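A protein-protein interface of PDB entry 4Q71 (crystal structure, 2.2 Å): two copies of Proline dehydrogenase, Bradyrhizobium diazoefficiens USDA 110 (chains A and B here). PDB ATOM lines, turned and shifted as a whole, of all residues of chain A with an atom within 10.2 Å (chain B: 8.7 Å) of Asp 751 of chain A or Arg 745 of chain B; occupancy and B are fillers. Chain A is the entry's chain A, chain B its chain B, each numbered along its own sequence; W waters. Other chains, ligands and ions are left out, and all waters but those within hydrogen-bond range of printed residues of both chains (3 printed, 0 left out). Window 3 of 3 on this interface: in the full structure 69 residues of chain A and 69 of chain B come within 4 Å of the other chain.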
ATOM      1  N   THR A 723      15.754  -6.516   7.627  1.00  0.00           N
ATOM      2  CA  THR A 723      16.743  -7.402   8.248  1.00  0.00           C
ATOM      3  C   THR A 723      16.921  -7.158   9.741  1.00  0.00           C
ATOM      4  O   THR A 723      17.547  -7.960  10.440  1.00  0.00           O
ATOM      5  CB  THR A 723      18.127  -7.310   7.569  1.00  0.00           C
ATOM      6  OG1 THR A 723      18.694  -6.011   7.795  1.00  0.00           O
ATOM      7  CG2 THR A 723      18.011  -7.564   6.072  1.00  0.00           C
ATOM      8  N   ALA A 724      16.367  -6.055  10.229  1.00  0.00           N
ATOM      9  CA  ALA A 724      16.419  -5.776  11.654  1.00  0.00           C
ATOM     10  C   ALA A 724      15.160  -6.296  12.343  1.00  0.00           C
ATOM     11  O   ALA A 724      15.118  -6.380  13.558  1.00  0.00           O
ATOM     12  CB  ALA A 724      16.605  -4.275  11.911  1.00  0.00           C
ATOM     13  N   HIS A 725      14.133  -6.636  11.566  1.00  0.00           N
ATOM     14  CA  HIS A 725      12.890  -7.156  12.139  1.00  0.00           C
ATOM     15  C   HIS A 725      13.112  -8.399  12.992  1.00  0.00           C
ATOM     16  O   HIS A 725      13.727  -9.367  12.538  1.00  0.00           O
ATOM     17  CB  HIS A 725      11.871  -7.477  11.044  1.00  0.00           C
ATOM     18  CG  HIS A 725      10.459  -7.523  11.537  1.00  0.00           C
ATOM     19  ND1 HIS A 725       9.998  -8.505  12.390  1.00  0.00           N
ATOM     20  CD2 HIS A 725       9.406  -6.704  11.307  1.00  0.00           C
ATOM     21  CE1 HIS A 725       8.723  -8.287  12.664  1.00  0.00           C
ATOM     22  NE2 HIS A 725       8.340  -7.200  12.020  1.00  0.00           N
ATOM     23  N   PRO A 726      12.579  -8.388  14.227  1.00  0.00           N
ATOM     24  CA  PRO A 726      12.791  -9.508  15.154  1.00  0.00           C
ATOM     25  C   PRO A 726      12.105 -10.815  14.758  1.00  0.00           C
ATOM     26  O   PRO A 726      12.506 -11.856  15.290  1.00  0.00           O
ATOM     27  CB  PRO A 726      12.185  -8.992  16.477  1.00  0.00           C
ATOM     28  CG  PRO A 726      11.171  -7.965  16.055  1.00  0.00           C
ATOM     29  CD  PRO A 726      11.817  -7.291  14.855  1.00  0.00           C
ATOM     30  N   ASP A 727      11.127 -10.779  13.853  1.00  0.00           N
ATOM     31  CA  ASP A 727      10.359 -11.987  13.518  1.00  0.00           C
ATOM     32  C   ASP A 727      10.822 -12.781  12.287  1.00  0.00           C
ATOM     33  O   ASP A 727      10.218 -13.796  11.942  1.00  0.00           O
ATOM     34  CB  ASP A 727       8.883 -11.653  13.361  1.00  0.00           C
ATOM     35  CG  ASP A 727       8.249 -11.212  14.659  1.00  0.00           C
ATOM     36  OD1 ASP A 727       8.885 -11.399  15.724  1.00  0.00           O
ATOM     37  OD2 ASP A 727       7.105 -10.708  14.606  1.00  0.00           O
ATOM     38  N   ARG A 741      28.134  -7.497   5.741  1.00  0.00           N
ATOM     39  CA  ARG A 741      28.623  -7.397   7.107  1.00  0.00           C
ATOM     40  C   ARG A 741      27.698  -6.571   7.971  1.00  0.00           C
ATOM     41  O   ARG A 741      27.454  -6.927   9.125  1.00  0.00           O
ATOM     42  CB  ARG A 741      30.028  -6.790   7.151  1.00  0.00           C
ATOM     43  CG  ARG A 741      31.117  -7.719   6.661  1.00  0.00           C
ATOM     44  CD  ARG A 741      32.467  -7.168   7.066  1.00  0.00           C
ATOM     45  NE  ARG A 741      32.737  -5.886   6.418  1.00  0.00           N
ATOM     46  CZ  ARG A 741      33.535  -5.751   5.364  1.00  0.00           C
ATOM     47  NH1 ARG A 741      34.132  -6.820   4.857  1.00  0.00           N
ATOM     48  NH2 ARG A 741      33.733  -4.558   4.820  1.00  0.00           N
ATOM     49  N   SER A 742      27.163  -5.484   7.422  1.00  0.00           N
ATOM     50  CA  SER A 742      26.235  -4.668   8.204  1.00  0.00           C
ATOM     51  C   SER A 742      24.954  -5.469   8.498  1.00  0.00           C
ATOM     52  O   SER A 742      24.412  -5.397   9.604  1.00  0.00           O
ATOM     53  CB  SER A 742      25.937  -3.323   7.523  1.00  0.00           C
ATOM     54  OG  SER A 742      24.818  -3.398   6.659  1.00  0.00           O
ATOM     55  N   ILE A 743      24.490  -6.242   7.516  1.00  0.00           N
ATOM     56  CA  ILE A 743      23.365  -7.161   7.737  1.00  0.00           C
ATOM     57  C   ILE A 743      23.698  -8.195   8.815  1.00  0.00           C
ATOM     58  O   ILE A 743      22.930  -8.383   9.754  1.00  0.00           O
ATOM     59  CB  ILE A 743      22.942  -7.880   6.442  1.00  0.00           C
ATOM     60  CG1 ILE A 743      22.266  -6.886   5.493  1.00  0.00           C
ATOM     61  CG2 ILE A 743      21.982  -9.018   6.749  1.00  0.00           C
ATOM     62  CD1 ILE A 743      21.964  -7.450   4.118  1.00  0.00           C
ATOM     63  N   ASN A 744      24.868  -8.818   8.700  1.00  0.00           N
ATOM     64  CA  ASN A 744      25.315  -9.806   9.672  1.00  0.00           C
ATOM     65  C   ASN A 744      25.380  -9.216  11.088  1.00  0.00           C
ATOM     66  O   ASN A 744      24.993  -9.867  12.069  1.00  0.00           O
ATOM     67  CB  ASN A 744      26.678 -10.376   9.240  1.00  0.00           C
ATOM     68  CG  ASN A 744      27.003 -11.710   9.916  1.00  0.00           C
ATOM     69  OD1 ASN A 744      26.109 -12.514  10.198  1.00  0.00           O
ATOM     70  ND2 ASN A 744      28.290 -11.952  10.166  1.00  0.00           N
ATOM     71  N   ARG A 745      25.811  -7.959  11.185  1.00  0.00           N
ATOM     72  CA  ARG A 745      25.896  -7.288  12.480  1.00  0.00           C
ATOM     73  C   ARG A 745      24.514  -6.986  13.020  1.00  0.00           C
ATOM     74  O   ARG A 745      24.261  -7.169  14.214  1.00  0.00           O
ATOM     75  CB  ARG A 745      26.711  -6.001  12.376  1.00  0.00           C
ATOM     76  CG  ARG A 745      28.208  -6.239  12.461  1.00  0.00           C
ATOM     77  CD  ARG A 745      29.019  -5.137  11.808  1.00  0.00           C
ATOM     78  NE  ARG A 745      30.366  -5.616  11.502  1.00  0.00           N
ATOM     79  CZ  ARG A 745      31.216  -4.997  10.687  1.00  0.00           C
ATOM     80  NH1 ARG A 745      32.414  -5.524  10.450  1.00  0.00           N
ATOM     81  NH2 ARG A 745      30.861  -3.857  10.101  1.00  0.00           N
ATOM     82  N   ALA A 746      23.608  -6.551  12.147  1.00  0.00           N
ATOM     83  CA  ALA A 746      22.237  -6.300  12.589  1.00  0.00           C
ATOM     84  C   ALA A 746      21.553  -7.601  13.062  1.00  0.00           C
ATOM     85  O   ALA A 746      20.842  -7.604  14.061  1.00  0.00           O
ATOM     86  CB  ALA A 746      21.432  -5.617  11.494  1.00  0.00           C
ATOM     87  N   LEU A 747      21.787  -8.706  12.359  1.00  0.00           N
ATOM     88  CA  LEU A 747      21.254  -9.991  12.810  1.00  0.00           C
ATOM     89  C   LEU A 747      21.896 -10.411  14.149  1.00  0.00           C
ATOM     90  O   LEU A 747      21.204 -10.767  15.098  1.00  0.00           O
ATOM     91  CB  LEU A 747      21.449 -11.066  11.731  1.00  0.00           C
ATOM     92  CG  LEU A 747      20.693 -10.883  10.407  1.00  0.00           C
ATOM     93  CD1 LEU A 747      21.078 -11.967   9.397  1.00  0.00           C
ATOM     94  CD2 LEU A 747      19.192 -10.921  10.634  1.00  0.00           C
ATOM     95  N   ALA A 748      23.218 -10.302  14.244  1.00  0.00           N
ATOM     96  CA  ALA A 748      23.913 -10.742  15.451  1.00  0.00           C
ATOM     97  C   ALA A 748      23.563  -9.896  16.672  1.00  0.00           C
ATOM     98  O   ALA A 748      23.657 -10.365  17.809  1.00  0.00           O
ATOM     99  CB  ALA A 748      25.407 -10.733  15.233  1.00  0.00           C
ATOM    100  N   ALA A 749      23.142  -8.660  16.424  1.00  0.00           N
ATOM    101  CA  ALA A 749      22.824  -7.738  17.499  1.00  0.00           C
ATOM    102  C   ALA A 749      21.530  -8.127  18.210  1.00  0.00           C
ATOM    103  O   ALA A 749      21.346  -7.801  19.384  1.00  0.00           O
ATOM    104  CB  ALA A 749      22.734  -6.309  16.955  1.00  0.00           C
ATOM    105  N   LYS A 750      20.629  -8.817  17.513  1.00  0.00           N
ATOM    106  CA  LYS A 750      19.336  -9.181  18.111  1.00  0.00           C
ATOM    107  C   LYS A 750      19.532 -10.130  19.284  1.00  0.00           C
ATOM    108  O   LYS A 750      20.537 -10.854  19.341  1.00  0.00           O
ATOM    109  CB  LYS A 750      18.425  -9.841  17.077  1.00  0.00           C
ATOM    110  CG  LYS A 750      18.243  -9.035  15.809  1.00  0.00           C
ATOM    111  CD  LYS A 750      17.497  -9.842  14.762  1.00  0.00           C
ATOM    112  CE  LYS A 750      17.177  -8.994  13.550  1.00  0.00           C
ATOM    113  NZ  LYS A 750      16.403  -9.763  12.528  1.00  0.00           N
ATOM    114  N   ASP A 751      18.578 -10.133  20.213  1.00  0.00           N
ATOM    115  CA  ASP A 751      18.651 -11.019  21.365  1.00  0.00           C
ATOM    116  C   ASP A 751      17.912 -12.325  21.092  1.00  0.00           C
ATOM    117  O   ASP A 751      17.959 -13.265  21.892  1.00  0.00           O
ATOM    118  CB  ASP A 751      18.116 -10.337  22.629  1.00  0.00           C
ATOM    119  CG  ASP A 751      19.055  -9.266  23.154  1.00  0.00           C
ATOM    120  OD1 ASP A 751      20.188  -9.607  23.563  1.00  0.00           O
ATOM    121  OD2 ASP A 751      18.656  -8.083  23.163  1.00  0.00           O
ATOM    122  N   GLY A 752      17.214 -12.375  19.963  1.00  0.00           N
ATOM    123  CA  GLY A 752      16.500 -13.575  19.577  1.00  0.00           C
ATOM    124  C   GLY A 752      17.369 -14.707  19.042  1.00  0.00           C
ATOM    125  O   GLY A 752      18.572 -14.784  19.324  1.00  0.00           O
ATOM    126  N   PRO A 753      16.753 -15.601  18.247  1.00  0.00           N
ATOM    127  CA  PRO A 753      17.447 -16.723  17.602  1.00  0.00           C
ATOM    128  C   PRO A 753      18.553 -16.253  16.673  1.00  0.00           C
ATOM    129  O   PRO A 753      18.423 -15.182  16.064  1.00  0.00           O
ATOM    130  CB  PRO A 753      16.348 -17.370  16.757  1.00  0.00           C
ATOM    131  CG  PRO A 753      15.060 -16.987  17.455  1.00  0.00           C
ATOM    132  CD  PRO A 753      15.303 -15.604  17.976  1.00  0.00           C
ATOM    133  N   ILE A 754      19.633 -17.032  16.597  1.00  0.00           N
ATOM    134  CA  ILE A 754      20.678 -16.820  15.604  1.00  0.00           C
ATOM    135  C   ILE A 754      20.128 -17.441  14.338  1.00  0.00           C
ATOM    136  O   ILE A 754      19.832 -18.633  14.311  1.00  0.00           O
ATOM    137  CB  ILE A 754      22.019 -17.491  16.015  1.00  0.00           C
ATOM    138  CG1 ILE A 754      22.582 -16.819  17.276  1.00  0.00           C
ATOM    139  CG2 ILE A 754      23.045 -17.451  14.872  1.00  0.00           C
ATOM    140  CD1 ILE A 754      23.808 -17.504  17.878  1.00  0.00           C
ATOM    141  N   VAL A 755      19.928 -16.621  13.315  1.00  0.00           N
ATOM    142  CA  VAL A 755      19.288 -17.077  12.093  1.00  0.00           C
ATOM    143  C   VAL A 755      20.346 -17.179  11.011  1.00  0.00           C
ATOM    144  O   VAL A 755      21.387 -16.553  11.124  1.00  0.00           O
ATOM    145  CB  VAL A 755      18.134 -16.141  11.668  1.00  0.00           C
ATOM    146  CG1 VAL A 755      17.095 -16.051  12.802  1.00  0.00           C
ATOM    147  CG2 VAL A 755      18.667 -14.757  11.286  1.00  0.00           C
ATOM    148  N   THR B 723      37.819 -16.904  19.563  1.00  0.00           N
ATOM    149  CA  THR B 723      36.744 -16.563  18.626  1.00  0.00           C
ATOM    150  C   THR B 723      36.849 -15.158  18.046  1.00  0.00           C
ATOM    151  O   THR B 723      36.157 -14.828  17.081  1.00  0.00           O
ATOM    152  CB  THR B 723      35.341 -16.721  19.267  1.00  0.00           C
ATOM    153  OG1 THR B 723      35.163 -15.746  20.303  1.00  0.00           O
ATOM    154  CG2 THR B 723      35.186 -18.104  19.846  1.00  0.00           C
ATOM    155  N   ALA B 724      37.717 -14.335  18.621  1.00  0.00           N
ATOM    156  CA  ALA B 724      37.933 -12.996  18.093  1.00  0.00           C
ATOM    157  C   ALA B 724      39.103 -13.006  17.121  1.00  0.00           C
ATOM    158  O   ALA B 724      39.306 -12.051  16.373  1.00  0.00           O
ATOM    159  CB  ALA B 724      38.170 -11.989  19.227  1.00  0.00           C
ATOM    160  N   THR B 737      22.996 -19.790  25.828  1.00  0.00           N
ATOM    161  CA  THR B 737      22.440 -18.905  24.818  1.00  0.00           C
ATOM    162  C   THR B 737      23.141 -17.553  24.802  1.00  0.00           C
ATOM    163  O   THR B 737      23.465 -17.026  23.729  1.00  0.00           O
ATOM    164  CB  THR B 737      20.921 -18.720  25.029  1.00  0.00           C
ATOM    165  OG1 THR B 737      20.233 -19.876  24.538  1.00  0.00           O
ATOM    166  CG2 THR B 737      20.415 -17.512  24.286  1.00  0.00           C
ATOM    167  N   GLU B 738      23.408 -17.013  25.989  1.00  0.00           N
ATOM    168  CA  GLU B 738      24.039 -15.704  26.101  1.00  0.00           C
ATOM    169  C   GLU B 738      25.449 -15.723  25.522  1.00  0.00           C
ATOM    170  O   GLU B 738      25.897 -14.749  24.905  1.00  0.00           O
ATOM    171  CB  GLU B 738      24.079 -15.232  27.562  1.00  0.00           C
ATOM    172  N   VAL B 739      26.158 -16.824  25.734  1.00  0.00           N
ATOM    173  CA  VAL B 739      27.537 -16.897  25.266  1.00  0.00           C
ATOM    174  C   VAL B 739      27.580 -17.075  23.738  1.00  0.00           C
ATOM    175  O   VAL B 739      28.451 -16.515  23.070  1.00  0.00           O
ATOM    176  CB  VAL B 739      28.338 -17.994  26.014  1.00  0.00           C
ATOM    177  CG1 VAL B 739      29.659 -18.286  25.305  1.00  0.00           C
ATOM    178  CG2 VAL B 739      28.584 -17.564  27.471  1.00  0.00           C
ATOM    179  N   ALA B 740      26.608 -17.805  23.196  1.00  0.00           N
ATOM    180  CA  ALA B 740      26.499 -18.001  21.748  1.00  0.00           C
ATOM    181  C   ALA B 740      26.332 -16.667  21.029  1.00  0.00           C
ATOM    182  O   ALA B 740      26.984 -16.408  20.017  1.00  0.00           O
ATOM    183  CB  ALA B 740      25.335 -18.931  21.419  1.00  0.00           C
ATOM    184  N   ARG B 741      25.468 -15.816  21.568  1.00  0.00           N
ATOM    185  CA  ARG B 741      25.243 -14.489  21.001  1.00  0.00           C
ATOM    186  C   ARG B 741      26.473 -13.610  21.082  1.00  0.00           C
ATOM    187  O   ARG B 741      26.771 -12.873  20.143  1.00  0.00           O
ATOM    188  CB  ARG B 741      24.093 -13.785  21.720  1.00  0.00           C
ATOM    189  CG  ARG B 741      22.718 -14.338  21.400  1.00  0.00           C
ATOM    190  CD  ARG B 741      21.678 -13.374  21.935  1.00  0.00           C
ATOM    191  NE  ARG B 741      21.733 -13.290  23.395  1.00  0.00           N
ATOM    192  CZ  ARG B 741      20.849 -13.866  24.200  1.00  0.00           C
ATOM    193  NH1 ARG B 741      19.833 -14.535  23.678  1.00  0.00           N
ATOM    194  NH2 ARG B 741      20.965 -13.750  25.517  1.00  0.00           N
ATOM    195  N   SER B 742      27.188 -13.687  22.197  1.00  0.00           N
ATOM    196  CA  SER B 742      28.396 -12.892  22.345  1.00  0.00           C
ATOM    197  C   SER B 742      29.439 -13.372  21.323  1.00  0.00           C
ATOM    198  O   SER B 742      30.076 -12.560  20.646  1.00  0.00           O
ATOM    199  CB  SER B 742      28.907 -12.917  23.799  1.00  0.00           C
ATOM    200  OG  SER B 742      29.771 -14.014  24.050  1.00  0.00           O
ATOM    201  N   ILE B 743      29.548 -14.690  21.156  1.00  0.00           N
ATOM    202  CA  ILE B 743      30.399 -15.252  20.099  1.00  0.00           C
ATOM    203  C   ILE B 743      29.938 -14.784  18.712  1.00  0.00           C
ATOM    204  O   ILE B 743      30.746 -14.310  17.917  1.00  0.00           O
ATOM    205  CB  ILE B 743      30.432 -16.797  20.145  1.00  0.00           C
ATOM    206  CG1 ILE B 743      31.179 -17.278  21.394  1.00  0.00           C
ATOM    207  CG2 ILE B 743      31.089 -17.363  18.900  1.00  0.00           C
ATOM    208  CD1 ILE B 743      31.131 -18.782  21.597  1.00  0.00           C
ATOM    209  N   ASN B 744      28.639 -14.886  18.443  1.00  0.00           N
ATOM    210  CA  ASN B 744      28.090 -14.456  17.158  1.00  0.00           C
ATOM    211  C   ASN B 744      28.349 -12.972  16.869  1.00  0.00           C
ATOM    212  O   ASN B 744      28.642 -12.602  15.730  1.00  0.00           O
ATOM    213  CB  ASN B 744      26.587 -14.773  17.090  1.00  0.00           C
ATOM    214  CG  ASN B 744      26.034 -14.730  15.657  1.00  0.00           C
ATOM    215  OD1 ASN B 744      26.734 -15.052  14.689  1.00  0.00           O
ATOM    216  ND2 ASN B 744      24.770 -14.328  15.525  1.00  0.00           N
ATOM    217  N   ARG B 745      28.281 -12.132  17.904  1.00  0.00           N
ATOM    218  CA  ARG B 745      28.520 -10.693  17.747  1.00  0.00           C
ATOM    219  C   ARG B 745      29.988 -10.407  17.489  1.00  0.00           C
ATOM    220  O   ARG B 745      30.336  -9.558  16.658  1.00  0.00           O
ATOM    221  CB  ARG B 745      28.044  -9.937  18.986  1.00  0.00           C
ATOM    222  CG  ARG B 745      26.546  -9.644  18.969  1.00  0.00           C
ATOM    223  CD  ARG B 745      25.948  -9.499  20.358  1.00  0.00           C
ATOM    224  NE  ARG B 745      24.497  -9.677  20.290  1.00  0.00           N
ATOM    225  CZ  ARG B 745      23.713  -9.901  21.340  1.00  0.00           C
ATOM    226  NH1 ARG B 745      22.403 -10.061  21.174  1.00  0.00           N
ATOM    227  NH2 ARG B 745      24.244  -9.969  22.555  1.00  0.00           N
ATOM    228  N   ALA B 746      30.853 -11.127  18.195  1.00  0.00           N
ATOM    229  CA  ALA B 746      32.288 -10.995  17.974  1.00  0.00           C
ATOM    230  C   ALA B 746      32.663 -11.430  16.553  1.00  0.00           C
ATOM    231  O   ALA B 746      33.498 -10.796  15.920  1.00  0.00           O
ATOM    232  CB  ALA B 746      33.070 -11.783  19.015  1.00  0.00           C
ATOM    233  N   LEU B 747      32.041 -12.494  16.043  1.00  0.00           N
ATOM    234  CA  LEU B 747      32.303 -12.905  14.661  1.00  0.00           C
ATOM    235  C   LEU B 747      31.815 -11.824  13.698  1.00  0.00           C
ATOM    236  O   LEU B 747      32.547 -11.397  12.807  1.00  0.00           O
ATOM    237  CB  LEU B 747      31.656 -14.269  14.352  1.00  0.00           C
ATOM    238  CG  LEU B 747      32.206 -15.465  15.146  1.00  0.00           C
ATOM    239  CD1 LEU B 747      31.428 -16.751  14.864  1.00  0.00           C
ATOM    240  CD2 LEU B 747      33.668 -15.689  14.837  1.00  0.00           C
ATOM    241  N   ALA B 748      30.603 -11.329  13.916  1.00  0.00           N
ATOM    242  CA  ALA B 748      30.020 -10.353  13.000  1.00  0.00           C
ATOM    243  C   ALA B 748      30.760  -9.020  13.013  1.00  0.00           C
ATOM    244  O   ALA B 748      30.751  -8.278  12.019  1.00  0.00           O
ATOM    245  CB  ALA B 748      28.552 -10.136  13.327  1.00  0.00           C
ATOM    246  N   ALA B 749      31.419  -8.731  14.129  1.00  0.00           N
ATOM    247  CA  ALA B 749      32.109  -7.461  14.279  1.00  0.00           C
ATOM    248  C   ALA B 749      33.365  -7.405  13.410  1.00  0.00           C
ATOM    249  O   ALA B 749      33.797  -6.321  13.020  1.00  0.00           O
ATOM    250  CB  ALA B 749      32.447  -7.212  15.758  1.00  0.00           C
ATOM    251  N   LYS B 750      33.957  -8.562  13.104  1.00  0.00           N
ATOM    252  CA  LYS B 750      35.192  -8.595  12.300  1.00  0.00           C
ATOM    253  C   LYS B 750      34.942  -8.076  10.889  1.00  0.00           C
ATOM    254  O   LYS B 750      33.814  -8.156  10.377  1.00  0.00           O
ATOM    255  CB  LYS B 750      35.752 -10.015  12.200  1.00  0.00           C
ATOM    256  CG  LYS B 750      35.971 -10.725  13.518  1.00  0.00           C
ATOM    257  CD  LYS B 750      36.349 -12.189  13.271  1.00  0.00           C
ATOM    258  CE  LYS B 750      36.671 -12.902  14.577  1.00  0.00           C
ATOM    259  NZ  LYS B 750      37.064 -14.339  14.386  1.00  0.00           N
ATOM    260  N   LEU B 757      28.842 -20.211  12.160  1.00  0.00           N
ATOM    261  CA  LEU B 757      28.695 -20.500  13.581  1.00  0.00           C
ATOM    262  C   LEU B 757      27.713 -21.657  13.774  1.00  0.00           C
ATOM    263  O   LEU B 757      26.538 -21.559  13.401  1.00  0.00           O
ATOM    264  CB  LEU B 757      28.213 -19.264  14.359  1.00  0.00           C
ATOM    265  CG  LEU B 757      27.907 -19.482  15.848  1.00  0.00           C
ATOM    266  CD1 LEU B 757      29.125 -19.970  16.625  1.00  0.00           C
ATOM    267  CD2 LEU B 757      27.322 -18.220  16.504  1.00  0.00           C
ATOM    268  N   THR B 912       8.088 -19.441  24.526  1.00  0.00           N
ATOM    269  CA  THR B 912       9.444 -19.319  25.078  1.00  0.00           C
ATOM    270  C   THR B 912      10.483 -18.968  24.005  1.00  0.00           C
ATOM    271  O   THR B 912      11.470 -18.301  24.304  1.00  0.00           O
ATOM    272  CB  THR B 912       9.925 -20.605  25.801  1.00  0.00           C
ATOM    273  OG1 THR B 912      10.280 -21.607  24.835  1.00  0.00           O
ATOM    274  CG2 THR B 912       8.864 -21.135  26.777  1.00  0.00           C
ATOM    275  N   TYR B 914      12.261 -21.228  22.579  1.00  0.00           N
ATOM    276  CA  TYR B 914      13.153 -22.386  22.529  1.00  0.00           C
ATOM    277  C   TYR B 914      12.558 -23.485  21.643  1.00  0.00           C
ATOM    278  O   TYR B 914      11.405 -23.393  21.218  1.00  0.00           O
ATOM    279  CB  TYR B 914      13.443 -22.906  23.950  1.00  0.00           C
ATOM    280  CG  TYR B 914      14.407 -22.021  24.749  1.00  0.00           C
ATOM    281  CD1 TYR B 914      15.788 -22.193  24.645  1.00  0.00           C
ATOM    282  CD2 TYR B 914      13.941 -21.021  25.595  1.00  0.00           C
ATOM    283  CE1 TYR B 914      16.678 -21.398  25.361  1.00  0.00           C
ATOM    284  CE2 TYR B 914      14.829 -20.212  26.325  1.00  0.00           C
ATOM    285  CZ  TYR B 914      16.195 -20.408  26.203  1.00  0.00           C
ATOM    286  OH  TYR B 914      17.082 -19.623  26.915  1.00  0.00           O
ATOM    287  N   GLY B 960      15.308 -22.167  16.872  1.00  0.00           N
ATOM    288  CA  GLY B 960      14.976 -20.982  17.643  1.00  0.00           C
ATOM    289  C   GLY B 960      16.123 -20.660  18.583  1.00  0.00           C
ATOM    290  O   GLY B 960      17.293 -20.743  18.179  1.00  0.00           O
ATOM    291  N   LEU B 961      15.800 -20.348  19.840  1.00  0.00           N
ATOM    292  CA  LEU B 961      16.804 -20.035  20.852  1.00  0.00           C
ATOM    293  C   LEU B 961      17.671 -21.244  21.221  1.00  0.00           C
ATOM    294  O   LEU B 961      18.715 -21.089  21.864  1.00  0.00           O
ATOM    295  CB  LEU B 961      16.133 -19.486  22.116  1.00  0.00           C
ATOM    296  CG  LEU B 961      15.370 -18.166  21.995  1.00  0.00           C
ATOM    297  CD1 LEU B 961      14.757 -17.766  23.337  1.00  0.00           C
ATOM    298  CD2 LEU B 961      16.319 -17.096  21.520  1.00  0.00           C
HETATM  299  O   HOH W   1      16.785 -14.400  24.121  1.00  0.00           O
HETATM  300  O   HOH W   2      23.595 -13.169  18.171  1.00  0.00           O
HETATM  301  O   HOH W   3      27.959 -13.848  12.949  1.00  0.00           O
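NE of Arg 745 of chain A sits at hydrogen-bond distance from O of Ala 748 of chain B. NH1 of Arg 745 of chain A lies within hydrogen-bond range of O of Ala 749 of chain B, 3.0 Å away. NH1 of Arg 745 of chain A is in hydrogen-bond range of O of Lys 750 of chain B (3.0 Å). The backbone carbonyl oxygen of Ala 748 of chain A is in hydrogen-bond range of the guanidinium group of Arg 745 of chain B (2.7 Å). The backbone carbonyl oxygen (O) of Ala 749 of chain A lies within hydrogen-bond range of the guanidinium group (NH1) of Arg 745 of chain B, at 3.1 Å. O of Lys 750 of chain A sits at hydrogen-bond distance from NH1 of Arg 745 of chain B, 2.7 Å away. NE of Arg 741 of chain B lies within salt-bridge range of OD1 of Asp 751 of chain A, 3.997 Å away. The guanidinium group of Arg 745 of chain B is in salt-bridge range of the side-chain carboxylate of Asp 751 of chain A, 3.3 Å away.
O of Thr 723 of chain A sits at hydrogen-bond distance from NZ of Lys 750 of chain A (3.0 Å). The backbone carbonyl oxygen (O) of His 725 of chain A sits at hydrogen-bond distance from the side-chain amino group (NZ) of Lys 750 of chain A, at 2.7 Å. O of Leu 961 of chain B lies within hydrogen-bond range of OG1 of Thr 737 of chain B (3.3 Å).
Asn 744 of chain A touches Ala 748 of chain B. O of Lys 750 of chain A touches CD of Arg 741 of chain B, at 3.8 Å. Gly 960 of chain B touches Pro 753 of chain A. Pro 753 of chain A touches Leu 961 of chain B. Ile 754 of chain A touches Ala 740 of chain B (CD1 to O, 3.98 Å). Leu 757 of chain B touches Ile 754 of chain A (CD2 to CD1, 3.8 Å).
Leu 747 of chain A touches none of the printed residues of chain B. Of the printed residues of chain B, Ala 748 of chain A touches Asn 744 (3.7 Å), Arg 745 (2.7 Å) and Ala 748 (3.7 Å). Of chain B, only Leu 961 (3.6 Å) comes within 4 Å of Gly 752 of chain A. Glu 738 of chain B touches none of the printed residues of chain A. Of chain A, only Lys 750 (3.8 Å) and Asp 751 (2.9 Å) come within 4 Å of Arg 741 of chain B. Of chain A, only Ala 748 (3.7 Å) and Ile 754 (3.6 Å) come within 4 Å of Asn 744 of chain B. Of chain A, only Ala 748, Ala 749, Lys 750 and Asp 751 come within 4 Å of Arg 745 of chain B. Ala 746 of chain B touches none of the printed residues of chain A. The nearest residue of chain A that does not touch Arg 745 of chain B is Arg 745 of chain A (5.8 Å). The nearest printed residue of chain B that does not touch Ile 754 of chain A is Arg 741 of chain B (4.4 Å).
Of the 21 printed residues of chain B, 10 touch a printed residue of chain A. Of the 20 printed residues of chain A, 10 touch a printed residue of chain B. Hydrophobic or aromatic side chains of chain A that line the printed part of chain B: Ala 748, Pro 753 and Ile 754. Among the printed residues, 19 pairs touch across the chains. Among the printed residues, Asp or Glu carboxylates within 4 Å of a Lys or Arg side-chain nitrogen of the other chain: Asp 751 of chain A with Arg 741 of chain B and Asp 751 of chain A with Arg 745 of chain B.
Asn 744 of chain A touches Ala 748 of chain B, and with the chains exchanged Ala 748 of chain A touches Asn 744 of chain B. Arg 745 of chain A touches Lys 750 of chain B, and with the chains exchanged Lys 750 of chain A touches Arg 745 of chain B.
Water W3 lies within hydrogen-bond range of the side-chain amide oxygen (OD1) of Asn 744 of chain B (2.4 Å) and the side-chain amide nitrogen (ND2) of Asn 744 of chain A (3.4 Å). Water W1 bridges O of Asp 751 of chain A (2.8 Å) and NH1 of Arg 741 of chain B (3.1 Å).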
